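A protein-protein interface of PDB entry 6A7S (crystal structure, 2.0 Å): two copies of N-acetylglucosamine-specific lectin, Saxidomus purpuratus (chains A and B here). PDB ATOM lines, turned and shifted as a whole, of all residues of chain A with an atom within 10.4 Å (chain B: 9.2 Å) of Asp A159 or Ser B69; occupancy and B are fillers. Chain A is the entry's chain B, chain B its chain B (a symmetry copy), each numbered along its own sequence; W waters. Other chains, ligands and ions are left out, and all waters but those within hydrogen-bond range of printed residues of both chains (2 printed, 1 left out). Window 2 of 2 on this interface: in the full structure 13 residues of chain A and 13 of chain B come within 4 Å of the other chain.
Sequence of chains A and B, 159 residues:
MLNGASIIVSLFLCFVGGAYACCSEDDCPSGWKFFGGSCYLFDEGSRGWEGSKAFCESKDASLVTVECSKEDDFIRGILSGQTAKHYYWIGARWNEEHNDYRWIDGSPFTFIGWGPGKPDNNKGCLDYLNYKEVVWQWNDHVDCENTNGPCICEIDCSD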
ATOM      1  N   CYS A  22      -4.597 -23.469 -23.948  1.00  0.00           N
ATOM      2  CA  CYS A  22      -5.149 -24.786 -24.157  1.00  0.00           C
ATOM      3  C   CYS A  22      -6.630 -24.745 -23.820  1.00  0.00           C
ATOM      4  O   CYS A  22      -7.307 -25.766 -23.904  1.00  0.00           O
ATOM      5  CB  CYS A  22      -4.391 -25.794 -23.299  1.00  0.00           C
ATOM      6  SG  CYS A  22      -2.619 -25.808 -23.689  1.00  0.00           S
ATOM      7  N   CYS A  23      -7.148 -23.554 -23.461  1.00  0.00           N
ATOM      8  CA  CYS A  23      -8.563 -23.453 -23.121  1.00  0.00           C
ATOM      9  C   CYS A  23      -9.406 -23.538 -24.375  1.00  0.00           C
ATOM     10  O   CYS A  23      -8.991 -23.157 -25.449  1.00  0.00           O
ATOM     11  CB  CYS A  23      -8.938 -22.149 -22.411  1.00  0.00           C
ATOM     12  SG  CYS A  23      -8.010 -21.832 -20.899  1.00  0.00           S
ATOM     13  N   SER A  24     -10.620 -24.037 -24.173  1.00  0.00           N
ATOM     14  CA  SER A  24     -11.713 -23.951 -25.076  1.00  0.00           C
ATOM     15  C   SER A  24     -12.812 -23.101 -24.417  1.00  0.00           C
ATOM     16  O   SER A  24     -12.780 -22.857 -23.191  1.00  0.00           O
ATOM     17  CB  SER A  24     -12.206 -25.371 -25.407  1.00  0.00           C
ATOM     18  OG  SER A  24     -11.124 -26.144 -25.914  1.00  0.00           O
ATOM     19  N   ASP A  27     -14.304 -24.244 -21.276  1.00  0.00           N
ATOM     20  CA  ASP A  27     -13.452 -24.280 -20.099  1.00  0.00           C
ATOM     21  C   ASP A  27     -13.586 -23.002 -19.250  1.00  0.00           C
ATOM     22  O   ASP A  27     -13.127 -22.993 -18.122  1.00  0.00           O
ATOM     23  CB  ASP A  27     -11.987 -24.470 -20.484  1.00  0.00           C
ATOM     24  CG  ASP A  27     -11.710 -25.842 -21.089  1.00  0.00           C
ATOM     25  OD1 ASP A  27     -12.412 -26.800 -20.708  1.00  0.00           O
ATOM     26  OD2 ASP A  27     -10.830 -25.943 -21.953  1.00  0.00           O
ATOM     27  N   GLY A  37      -7.335 -19.328 -26.893  1.00  0.00           N
ATOM     28  CA  GLY A  37      -6.825 -20.388 -26.059  1.00  0.00           C
ATOM     29  C   GLY A  37      -6.682 -20.002 -24.597  1.00  0.00           C
ATOM     30  O   GLY A  37      -6.165 -20.817 -23.804  1.00  0.00           O
ATOM     31  N   LYS A  59      -7.556 -16.607  -7.668  1.00  0.00           N
ATOM     32  CA  LYS A  59      -8.461 -17.268  -8.592  1.00  0.00           C
ATOM     33  C   LYS A  59      -7.768 -18.414  -9.335  1.00  0.00           C
ATOM     34  O   LYS A  59      -8.298 -18.836 -10.356  1.00  0.00           O
ATOM     35  CB  LYS A  59      -8.973 -16.270  -9.631  1.00  0.00           C
ATOM     36  CG  LYS A  59      -9.727 -15.095  -9.059  1.00  0.00           C
ATOM     37  CD  LYS A  59     -11.050 -15.519  -8.600  1.00  0.00           C
ATOM     38  CE  LYS A  59     -12.026 -14.384  -8.619  1.00  0.00           C
ATOM     39  NZ  LYS A  59     -13.368 -14.901  -8.305  1.00  0.00           N
ATOM     40  N   ASP A  60      -6.605 -18.863  -8.841  1.00  0.00           N
ATOM     41  CA  ASP A  60      -5.773 -19.895  -9.507  1.00  0.00           C
ATOM     42  C   ASP A  60      -5.429 -19.376 -10.905  1.00  0.00           C
ATOM     43  O   ASP A  60      -5.614 -20.037 -11.915  1.00  0.00           O
ATOM     44  CB  ASP A  60      -6.516 -21.232  -9.591  1.00  0.00           C
ATOM     45  CG  ASP A  60      -6.832 -21.728  -8.204  1.00  0.00           C
ATOM     46  OD1 ASP A  60      -5.920 -21.670  -7.386  1.00  0.00           O
ATOM     47  OD2 ASP A  60      -7.997 -22.013  -7.939  1.00  0.00           O
ATOM     48  N   ALA A  61      -4.936 -18.144 -10.944  1.00  0.00           N
ATOM     49  CA  ALA A  61      -4.803 -17.473 -12.202  1.00  0.00           C
ATOM     50  C   ALA A  61      -3.696 -16.453 -12.026  1.00  0.00           C
ATOM     51  O   ALA A  61      -3.008 -16.482 -11.015  1.00  0.00           O
ATOM     52  CB  ALA A  61      -6.142 -16.914 -12.623  1.00  0.00           C
ATOM     53  N   ILE A 155      -6.216 -17.284 -17.491  1.00  0.00           N
ATOM     54  CA  ILE A 155      -5.834 -18.714 -17.396  1.00  0.00           C
ATOM     55  C   ILE A 155      -5.686 -19.288 -18.810  1.00  0.00           C
ATOM     56  O   ILE A 155      -6.429 -18.945 -19.737  1.00  0.00           O
ATOM     57  CB  ILE A 155      -6.861 -19.531 -16.584  1.00  0.00           C
ATOM     58  CG1 ILE A 155      -8.248 -19.567 -17.228  1.00  0.00           C
ATOM     59  CG2 ILE A 155      -6.889 -19.007 -15.154  1.00  0.00           C
ATOM     60  CD1 ILE A 155      -9.265 -20.528 -16.568  1.00  0.00           C
ATOM     61  N   ASP A 156      -4.791 -20.254 -18.938  1.00  0.00           N
ATOM     62  CA  ASP A 156      -4.660 -20.965 -20.205  1.00  0.00           C
ATOM     63  C   ASP A 156      -4.932 -22.481 -20.086  1.00  0.00           C
ATOM     64  O   ASP A 156      -4.587 -23.217 -20.975  1.00  0.00           O
ATOM     65  CB  ASP A 156      -3.276 -20.692 -20.738  1.00  0.00           C
ATOM     66  CG  ASP A 156      -2.195 -21.395 -19.960  1.00  0.00           C
ATOM     67  OD1 ASP A 156      -2.529 -22.132 -19.020  1.00  0.00           O
ATOM     68  OD2 ASP A 156      -1.040 -21.197 -20.324  1.00  0.00           O
ATOM     69  N   CYS A 157      -5.546 -22.937 -18.995  1.00  0.00           N
ATOM     70  CA  CYS A 157      -6.064 -24.307 -18.850  1.00  0.00           C
ATOM     71  C   CYS A 157      -4.994 -25.377 -19.148  1.00  0.00           C
ATOM     72  O   CYS A 157      -5.318 -26.429 -19.740  1.00  0.00           O
ATOM     73  CB  CYS A 157      -7.192 -24.576 -19.823  1.00  0.00           C
ATOM     74  SG  CYS A 157      -8.594 -23.465 -19.654  1.00  0.00           S
ATOM     75  N   SER A 158      -3.741 -25.088 -18.792  1.00  0.00           N
ATOM     76  CA  SER A 158      -2.608 -25.901 -19.113  1.00  0.00           C
ATOM     77  C   SER A 158      -2.371 -26.879 -17.956  1.00  0.00           C
ATOM     78  O   SER A 158      -1.371 -27.593 -17.944  1.00  0.00           O
ATOM     79  CB  SER A 158      -1.391 -25.087 -19.458  1.00  0.00           C
ATOM     80  OG  SER A 158      -1.068 -24.214 -18.403  1.00  0.00           O
ATOM     81  N   ASP A 159      -3.226 -26.740 -16.938  1.00  0.00           N
ATOM     82  CA  ASP A 159      -4.123 -27.773 -16.417  1.00  0.00           C
ATOM     83  C   ASP A 159      -4.806 -27.241 -15.156  1.00  0.00           C
ATOM     84  O   ASP A 159      -4.145 -27.229 -14.141  1.00  0.00           O
ATOM     85  CB  ASP A 159      -3.429 -29.113 -16.153  1.00  0.00           C
ATOM     86  CG  ASP A 159      -4.301 -30.269 -16.606  1.00  0.00           C
ATOM     87  OD1 ASP A 159      -5.299 -30.001 -17.332  1.00  0.00           O
ATOM     88  OD2 ASP A 159      -3.993 -31.419 -16.233  1.00  0.00           O
ATOM     89  N   PHE B  35      -7.836 -25.874 -32.103  1.00  0.00           N
ATOM     90  CA  PHE B  35      -7.956 -26.266 -30.713  1.00  0.00           C
ATOM     91  C   PHE B  35      -7.107 -25.337 -29.858  1.00  0.00           C
ATOM     92  O   PHE B  35      -5.916 -25.186 -30.097  1.00  0.00           O
ATOM     93  CB  PHE B  35      -7.474 -27.699 -30.445  1.00  0.00           C
ATOM     94  CG  PHE B  35      -7.420 -28.021 -28.979  1.00  0.00           C
ATOM     95  CD1 PHE B  35      -8.567 -28.412 -28.313  1.00  0.00           C
ATOM     96  CD2 PHE B  35      -6.264 -27.791 -28.234  1.00  0.00           C
ATOM     97  CE1 PHE B  35      -8.561 -28.619 -26.941  1.00  0.00           C
ATOM     98  CE2 PHE B  35      -6.262 -27.990 -26.858  1.00  0.00           C
ATOM     99  CZ  PHE B  35      -7.399 -28.438 -26.221  1.00  0.00           C
ATOM    100  N   VAL B  66       3.559 -29.766 -27.412  1.00  0.00           N
ATOM    101  CA  VAL B  66       2.409 -30.155 -26.638  1.00  0.00           C
ATOM    102  C   VAL B  66       2.580 -29.684 -25.189  1.00  0.00           C
ATOM    103  O   VAL B  66       3.321 -30.304 -24.401  1.00  0.00           O
ATOM    104  CB  VAL B  66       2.100 -31.657 -26.741  1.00  0.00           C
ATOM    105  CG1 VAL B  66       0.790 -31.999 -26.060  1.00  0.00           C
ATOM    106  CG2 VAL B  66       2.057 -32.119 -28.187  1.00  0.00           C
ATOM    107  N   GLU B  67       1.901 -28.565 -24.860  1.00  0.00           N
ATOM    108  CA  GLU B  67       2.144 -27.867 -23.586  1.00  0.00           C
ATOM    109  C   GLU B  67       1.216 -28.380 -22.494  1.00  0.00           C
ATOM    110  O   GLU B  67       1.445 -28.056 -21.334  1.00  0.00           O
ATOM    111  CB  GLU B  67       1.943 -26.350 -23.690  1.00  0.00           C
ATOM    112  CG  GLU B  67       3.068 -25.668 -24.453  1.00  0.00           C
ATOM    113  CD  GLU B  67       3.067 -25.833 -25.960  1.00  0.00           C
ATOM    114  OE1 GLU B  67       1.973 -26.122 -26.620  1.00  0.00           O
ATOM    115  OE2 GLU B  67       4.167 -25.693 -26.520  1.00  0.00           O
ATOM    116  N   CYS B  68       0.177 -29.140 -22.844  1.00  0.00           N
ATOM    117  CA  CYS B  68      -0.769 -29.487 -21.801  1.00  0.00           C
ATOM    118  C   CYS B  68      -1.637 -30.705 -22.149  1.00  0.00           C
ATOM    119  O   CYS B  68      -1.744 -31.088 -23.307  1.00  0.00           O
ATOM    120  CB  CYS B  68      -1.690 -28.312 -21.580  1.00  0.00           C
ATOM    121  SG  CYS B  68      -2.546 -27.945 -23.112  1.00  0.00           S
ATOM    122  N   SER B  69      -2.275 -31.289 -21.120  1.00  0.00           N
ATOM    123  CA  SER B  69      -2.873 -32.577 -21.276  1.00  0.00           C
ATOM    124  C   SER B  69      -4.111 -32.401 -22.136  1.00  0.00           C
ATOM    125  O   SER B  69      -4.454 -33.253 -22.876  1.00  0.00           O
ATOM    126  CB  SER B  69      -3.179 -33.249 -19.977  1.00  0.00           C
ATOM    127  OG  SER B  69      -4.324 -32.653 -19.434  1.00  0.00           O
ATOM    128  N   LYS B  70      -4.714 -31.215 -22.138  1.00  0.00           N
ATOM    129  CA  LYS B  70      -5.903 -31.049 -23.027  1.00  0.00           C
ATOM    130  C   LYS B  70      -5.533 -31.087 -24.521  1.00  0.00           C
ATOM    131  O   LYS B  70      -6.298 -31.582 -25.334  1.00  0.00           O
ATOM    132  CB  LYS B  70      -6.608 -29.741 -22.698  1.00  0.00           C
ATOM    133  CG  LYS B  70      -7.401 -29.814 -21.406  1.00  0.00           C
ATOM    134  CD  LYS B  70      -8.047 -28.498 -21.038  1.00  0.00           C
ATOM    135  CE  LYS B  70      -8.418 -28.441 -19.581  1.00  0.00           C
ATOM    136  NZ  LYS B  70      -9.671 -29.196 -19.391  1.00  0.00           N
ATOM    137  N   GLU B  71      -4.366 -30.541 -24.854  1.00  0.00           N
ATOM    138  CA  GLU B  71      -3.833 -30.532 -26.189  1.00  0.00           C
ATOM    139  C   GLU B  71      -3.369 -31.955 -26.551  1.00  0.00           C
ATOM    140  O   GLU B  71      -3.594 -32.396 -27.607  1.00  0.00           O
ATOM    141  CB  GLU B  71      -2.639 -29.593 -26.302  1.00  0.00           C
ATOM    142  CG  GLU B  71      -2.120 -29.378 -27.721  1.00  0.00           C
ATOM    143  CD  GLU B  71      -0.973 -28.367 -27.846  1.00  0.00           C
ATOM    144  OE1 GLU B  71      -0.236 -28.150 -26.874  1.00  0.00           O
ATOM    145  OE2 GLU B  71      -0.782 -27.838 -28.941  1.00  0.00           O
ATOM    146  N   ASP B  72      -2.687 -32.612 -25.642  1.00  0.00           N
ATOM    147  CA  ASP B  72      -2.366 -34.025 -25.824  1.00  0.00           C
ATOM    148  C   ASP B  72      -3.631 -34.813 -26.186  1.00  0.00           C
ATOM    149  O   ASP B  72      -3.643 -35.667 -27.110  1.00  0.00           O
ATOM    150  CB  ASP B  72      -1.663 -34.527 -24.571  1.00  0.00           C
ATOM    151  CG  ASP B  72      -1.343 -36.015 -24.604  1.00  0.00           C
ATOM    152  OD1 ASP B  72      -0.376 -36.371 -25.273  1.00  0.00           O
ATOM    153  OD2 ASP B  72      -2.066 -36.776 -23.918  1.00  0.00           O
ATOM    154  N   ASP B  73      -4.714 -34.580 -25.472  1.00  0.00           N
ATOM    155  CA  ASP B  73      -5.911 -35.444 -25.671  1.00  0.00           C
ATOM    156  C   ASP B  73      -6.635 -35.006 -26.938  1.00  0.00           C
ATOM    157  O   ASP B  73      -7.231 -35.812 -27.649  1.00  0.00           O
ATOM    158  CB  ASP B  73      -6.859 -35.470 -24.462  1.00  0.00           C
ATOM    159  CG  ASP B  73      -7.689 -36.768 -24.355  1.00  0.00           C
ATOM    160  OD1 ASP B  73      -7.102 -37.880 -24.564  1.00  0.00           O
ATOM    161  OD2 ASP B  73      -8.911 -36.672 -24.092  1.00  0.00           O
ATOM    162  N   PHE B  74      -6.541 -33.712 -27.287  1.00  0.00           N
ATOM    163  CA  PHE B  74      -7.104 -33.255 -28.565  1.00  0.00           C
ATOM    164  C   PHE B  74      -6.428 -34.000 -29.743  1.00  0.00           C
ATOM    165  O   PHE B  74      -7.101 -34.591 -30.627  1.00  0.00           O
ATOM    166  CB  PHE B  74      -6.948 -31.735 -28.723  1.00  0.00           C
ATOM    167  CG  PHE B  74      -7.119 -31.301 -30.151  1.00  0.00           C
ATOM    168  CD1 PHE B  74      -8.376 -31.307 -30.746  1.00  0.00           C
ATOM    169  CD2 PHE B  74      -6.013 -30.998 -30.922  1.00  0.00           C
ATOM    170  CE1 PHE B  74      -8.533 -30.919 -32.066  1.00  0.00           C
ATOM    171  CE2 PHE B  74      -6.173 -30.594 -32.247  1.00  0.00           C
ATOM    172  CZ  PHE B  74      -7.432 -30.570 -32.811  1.00  0.00           C
ATOM    173  N   ILE B  75      -5.102 -34.057 -29.701  1.00  0.00           N
ATOM    174  CA  ILE B  75      -4.329 -34.769 -30.682  1.00  0.00           C
ATOM    175  C   ILE B  75      -4.718 -36.259 -30.681  1.00  0.00           C
ATOM    176  O   ILE B  75      -4.943 -36.839 -31.746  1.00  0.00           O
ATOM    177  CB  ILE B  75      -2.830 -34.582 -30.421  1.00  0.00           C
ATOM    178  CG1 ILE B  75      -2.361 -33.173 -30.798  1.00  0.00           C
ATOM    179  CG2 ILE B  75      -2.020 -35.628 -31.152  1.00  0.00           C
ATOM    180  CD1 ILE B  75      -1.016 -32.863 -30.214  1.00  0.00           C
ATOM    181  N   ARG B  76      -4.806 -36.861 -29.503  1.00  0.00           N
ATOM    182  CA  ARG B  76      -5.124 -38.304 -29.449  1.00  0.00           C
ATOM    183  C   ARG B  76      -6.481 -38.567 -30.122  1.00  0.00           C
ATOM    184  O   ARG B  76      -6.624 -39.475 -30.874  1.00  0.00           O
ATOM    185  CB  ARG B  76      -5.129 -38.753 -27.997  1.00  0.00           C
ATOM    186  CG  ARG B  76      -5.451 -40.233 -27.819  1.00  0.00           C
ATOM    187  CD  ARG B  76      -5.312 -40.625 -26.370  1.00  0.00           C
ATOM    188  NE  ARG B  76      -3.937 -40.466 -25.895  1.00  0.00           N
ATOM    189  CZ  ARG B  76      -3.494 -39.505 -25.108  1.00  0.00           C
ATOM    190  NH1 ARG B  76      -4.354 -38.705 -24.498  1.00  0.00           N
ATOM    191  NH2 ARG B  76      -2.186 -39.376 -24.912  1.00  0.00           N
ATOM    192  N   GLY B  77      -7.460 -37.703 -29.877  1.00  0.00           N
ATOM    193  CA  GLY B  77      -8.791 -37.826 -30.456  1.00  0.00           C
ATOM    194  C   GLY B  77      -8.770 -37.851 -31.971  1.00  0.00           C
ATOM    195  O   GLY B  77      -9.507 -38.616 -32.614  1.00  0.00           O
ATOM    196  N   THR B 110       6.587 -29.379 -20.205  1.00  0.00           N
ATOM    197  CA  THR B 110       5.827 -29.065 -19.064  1.00  0.00           C
ATOM    198  C   THR B 110       4.921 -30.254 -18.823  1.00  0.00           C
ATOM    199  O   THR B 110       5.239 -31.099 -18.027  1.00  0.00           O
ATOM    200  CB  THR B 110       5.072 -27.742 -19.259  1.00  0.00           C
ATOM    201  OG1 THR B 110       4.386 -27.714 -20.514  1.00  0.00           O
ATOM    202  CG2 THR B 110       6.013 -26.561 -19.191  1.00  0.00           C
ATOM    203  N   PHE B 111       3.850 -30.360 -19.608  1.00  0.00           N
ATOM    204  CA  PHE B 111       3.148 -31.644 -19.745  1.00  0.00           C
ATOM    205  C   PHE B 111       4.139 -32.746 -20.182  1.00  0.00           C
ATOM    206  O   PHE B 111       5.061 -32.528 -20.991  1.00  0.00           O
ATOM    207  CB  PHE B 111       1.952 -31.476 -20.674  1.00  0.00           C
ATOM    208  CG  PHE B 111       1.298 -32.786 -21.002  1.00  0.00           C
ATOM    209  CD1 PHE B 111       0.466 -33.402 -20.101  1.00  0.00           C
ATOM    210  CD2 PHE B 111       1.592 -33.429 -22.191  1.00  0.00           C
ATOM    211  CE1 PHE B 111      -0.102 -34.634 -20.388  1.00  0.00           C
ATOM    212  CE2 PHE B 111       1.022 -34.653 -22.482  1.00  0.00           C
ATOM    213  CZ  PHE B 111       0.178 -35.247 -21.585  1.00  0.00           C
ATOM    214  N   ILE B 112       4.015 -33.915 -19.551  1.00  0.00           N
ATOM    215  CA  ILE B 112       4.845 -35.072 -19.848  1.00  0.00           C
ATOM    216  C   ILE B 112       3.915 -36.130 -20.429  1.00  0.00           C
ATOM    217  O   ILE B 112       3.050 -36.597 -19.756  1.00  0.00           O
ATOM    218  CB  ILE B 112       5.565 -35.608 -18.587  1.00  0.00           C
ATOM    219  CG1 ILE B 112       6.386 -34.520 -17.887  1.00  0.00           C
ATOM    220  CG2 ILE B 112       6.427 -36.806 -18.927  1.00  0.00           C
ATOM    221  CD1 ILE B 112       7.472 -33.920 -18.729  1.00  0.00           C
ATOM    222  N   GLY B 113       4.133 -36.527 -21.677  1.00  0.00           N
ATOM    223  CA  GLY B 113       3.180 -37.378 -22.375  1.00  0.00           C
ATOM    224  C   GLY B 113       3.768 -38.710 -22.853  1.00  0.00           C
ATOM    225  O   GLY B 113       3.167 -39.384 -23.713  1.00  0.00           O
ATOM    226  N   TYR B 128       3.949 -39.343 -31.788  1.00  0.00           N
ATOM    227  CA  TYR B 128       2.864 -40.024 -31.165  1.00  0.00           C
ATOM    228  C   TYR B 128       2.857 -41.423 -31.747  1.00  0.00           C
ATOM    229  O   TYR B 128       2.980 -41.559 -32.944  1.00  0.00           O
ATOM    230  CB  TYR B 128       1.517 -39.338 -31.420  1.00  0.00           C
ATOM    231  CG  TYR B 128       1.222 -38.278 -30.402  1.00  0.00           C
ATOM    232  CD1 TYR B 128       1.695 -36.980 -30.569  1.00  0.00           C
ATOM    233  CD2 TYR B 128       0.524 -38.558 -29.252  1.00  0.00           C
ATOM    234  CE1 TYR B 128       1.467 -35.996 -29.621  1.00  0.00           C
ATOM    235  CE2 TYR B 128       0.270 -37.578 -28.299  1.00  0.00           C
ATOM    236  CZ  TYR B 128       0.765 -36.295 -28.472  1.00  0.00           C
ATOM    237  OH  TYR B 128       0.568 -35.333 -27.524  1.00  0.00           O
ATOM    238  N   TRP B 138       3.725 -40.480 -26.487  1.00  0.00           N
ATOM    239  CA  TRP B 138       4.967 -40.181 -27.115  1.00  0.00           C
ATOM    240  C   TRP B 138       5.966 -41.373 -27.043  1.00  0.00           C
ATOM    241  O   TRP B 138       6.006 -42.079 -26.053  1.00  0.00           O
ATOM    242  CB  TRP B 138       5.620 -38.984 -26.433  1.00  0.00           C
ATOM    243  CG  TRP B 138       4.797 -37.756 -26.252  1.00  0.00           C
ATOM    244  CD1 TRP B 138       3.645 -37.365 -26.868  1.00  0.00           C
ATOM    245  CD2 TRP B 138       5.207 -36.685 -25.411  1.00  0.00           C
ATOM    246  NE1 TRP B 138       3.277 -36.135 -26.414  1.00  0.00           N
ATOM    247  CE2 TRP B 138       4.224 -35.688 -25.528  1.00  0.00           C
ATOM    248  CE3 TRP B 138       6.285 -36.511 -24.536  1.00  0.00           C
ATOM    249  CZ2 TRP B 138       4.297 -34.519 -24.776  1.00  0.00           C
ATOM    250  CZ3 TRP B 138       6.373 -35.332 -23.825  1.00  0.00           C
ATOM    251  CH2 TRP B 138       5.373 -34.364 -23.932  1.00  0.00           C
HETATM  252  O   HOH W   1      -1.497 -30.346 -18.556  1.00  0.00           O
HETATM  253  O   HOH W   2       1.222 -27.746 -18.580  1.00  0.00           O
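Among the printed residues, merely in contact across the chains: Cys A22 with Phe B35 (3.5 Å), Ser A158 with Cys B68 (3.6 Å), Cys A157 with Lys B70 (3.7 Å) and Ser A24 with Phe B35 (3.7 Å).
SG of Cys A22 forms a disulfide with SG of Cys B68, at 2.2 Å. OD1 of Asp A27 lies within salt-bridge range of NZ of Lys B70. The side-chain carboxylate (OD2) of Asp A159 sits at hydrogen-bond distance from the side-chain hydroxyl (OG) of Ser B69 (3.4 Å).
Water W2 bridges O of Ser A158 (2.7 Å) and O of Glu B67 (2.8 Å). Water W1 lies within hydrogen-bond range of O of Ser A158 (2.8 Å) and N of Ser B69 (2.8 Å).
Of chain B, only Ser B69 (3.4 Å) comes within 4 Å of Asp A159. Ser B69 touches one residue of chain A. Ser A158 touches one residue of chain B. Of chain A, only Asp A27 (3.9 Å) and Cys A157 (3.7 Å) come within 4 Å of Lys B70. No residue of chain A comes within 4 Å of Asp B72. No residue of chain A comes within 4 Å of Asp B73. Printed residues of chain B within 4 Å of Cys A157: Lys B70. Of the printed residues of chain B, Asp A27 touches Lys B70. Printed residues of chain A within 4 Å of Phe B35: Cys A22 (3.5 Å) and Ser A24 (3.7 Å). Of the printed residues of chain B, Cys A22 touches Phe B35 (3.5 Å) and Cys B68 (2.2 Å). Printed residues of chain B within 4 Å of Ser A24: Phe B35 (3.7 Å). The nearest residue of chain B that does not touch Asp A159 is Lys B70 (4.1 Å). The nearest residue of chain A that does not touch Ser B69 is Ser A158 (5.0 Å). The nearest printed residue of chain B that does not touch Cys A157 is Cys B68 (4.5 Å).
No position is printed for both chains.
The backbone NH (N) of Cys A22 is in hydrogen-bond range of the backbone carbonyl oxygen (O) of Gly A37 (3.1 Å). O of Asp A156 is in hydrogen-bond range of N of Cys A22 (3.0 Å). The side-chain sulfur (SG) of Cys A157 is disulfide-bonded to the side-chain sulfur (SG) of Cys A23, 2.1 Å away. The backbone NH (N) of Ser A24 sits at hydrogen-bond distance from the side-chain carboxylate (OD2) of Asp A27 (2.9 Å). The side-chain hydroxyl (OG) of Ser A158 is in hydrogen-bond range of the side-chain carboxylate (OD1) of Asp A156 (2.6 Å). The backbone NH of Glu B71 lies close to the side-chain sulfur of Cys B68 (3.6 Å).
Hydrophobic or aromatic side chains of chain B within 4 Å of the printed part of chain A: Phe B35. Among the printed residues, 7 pairs touch across the chains.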
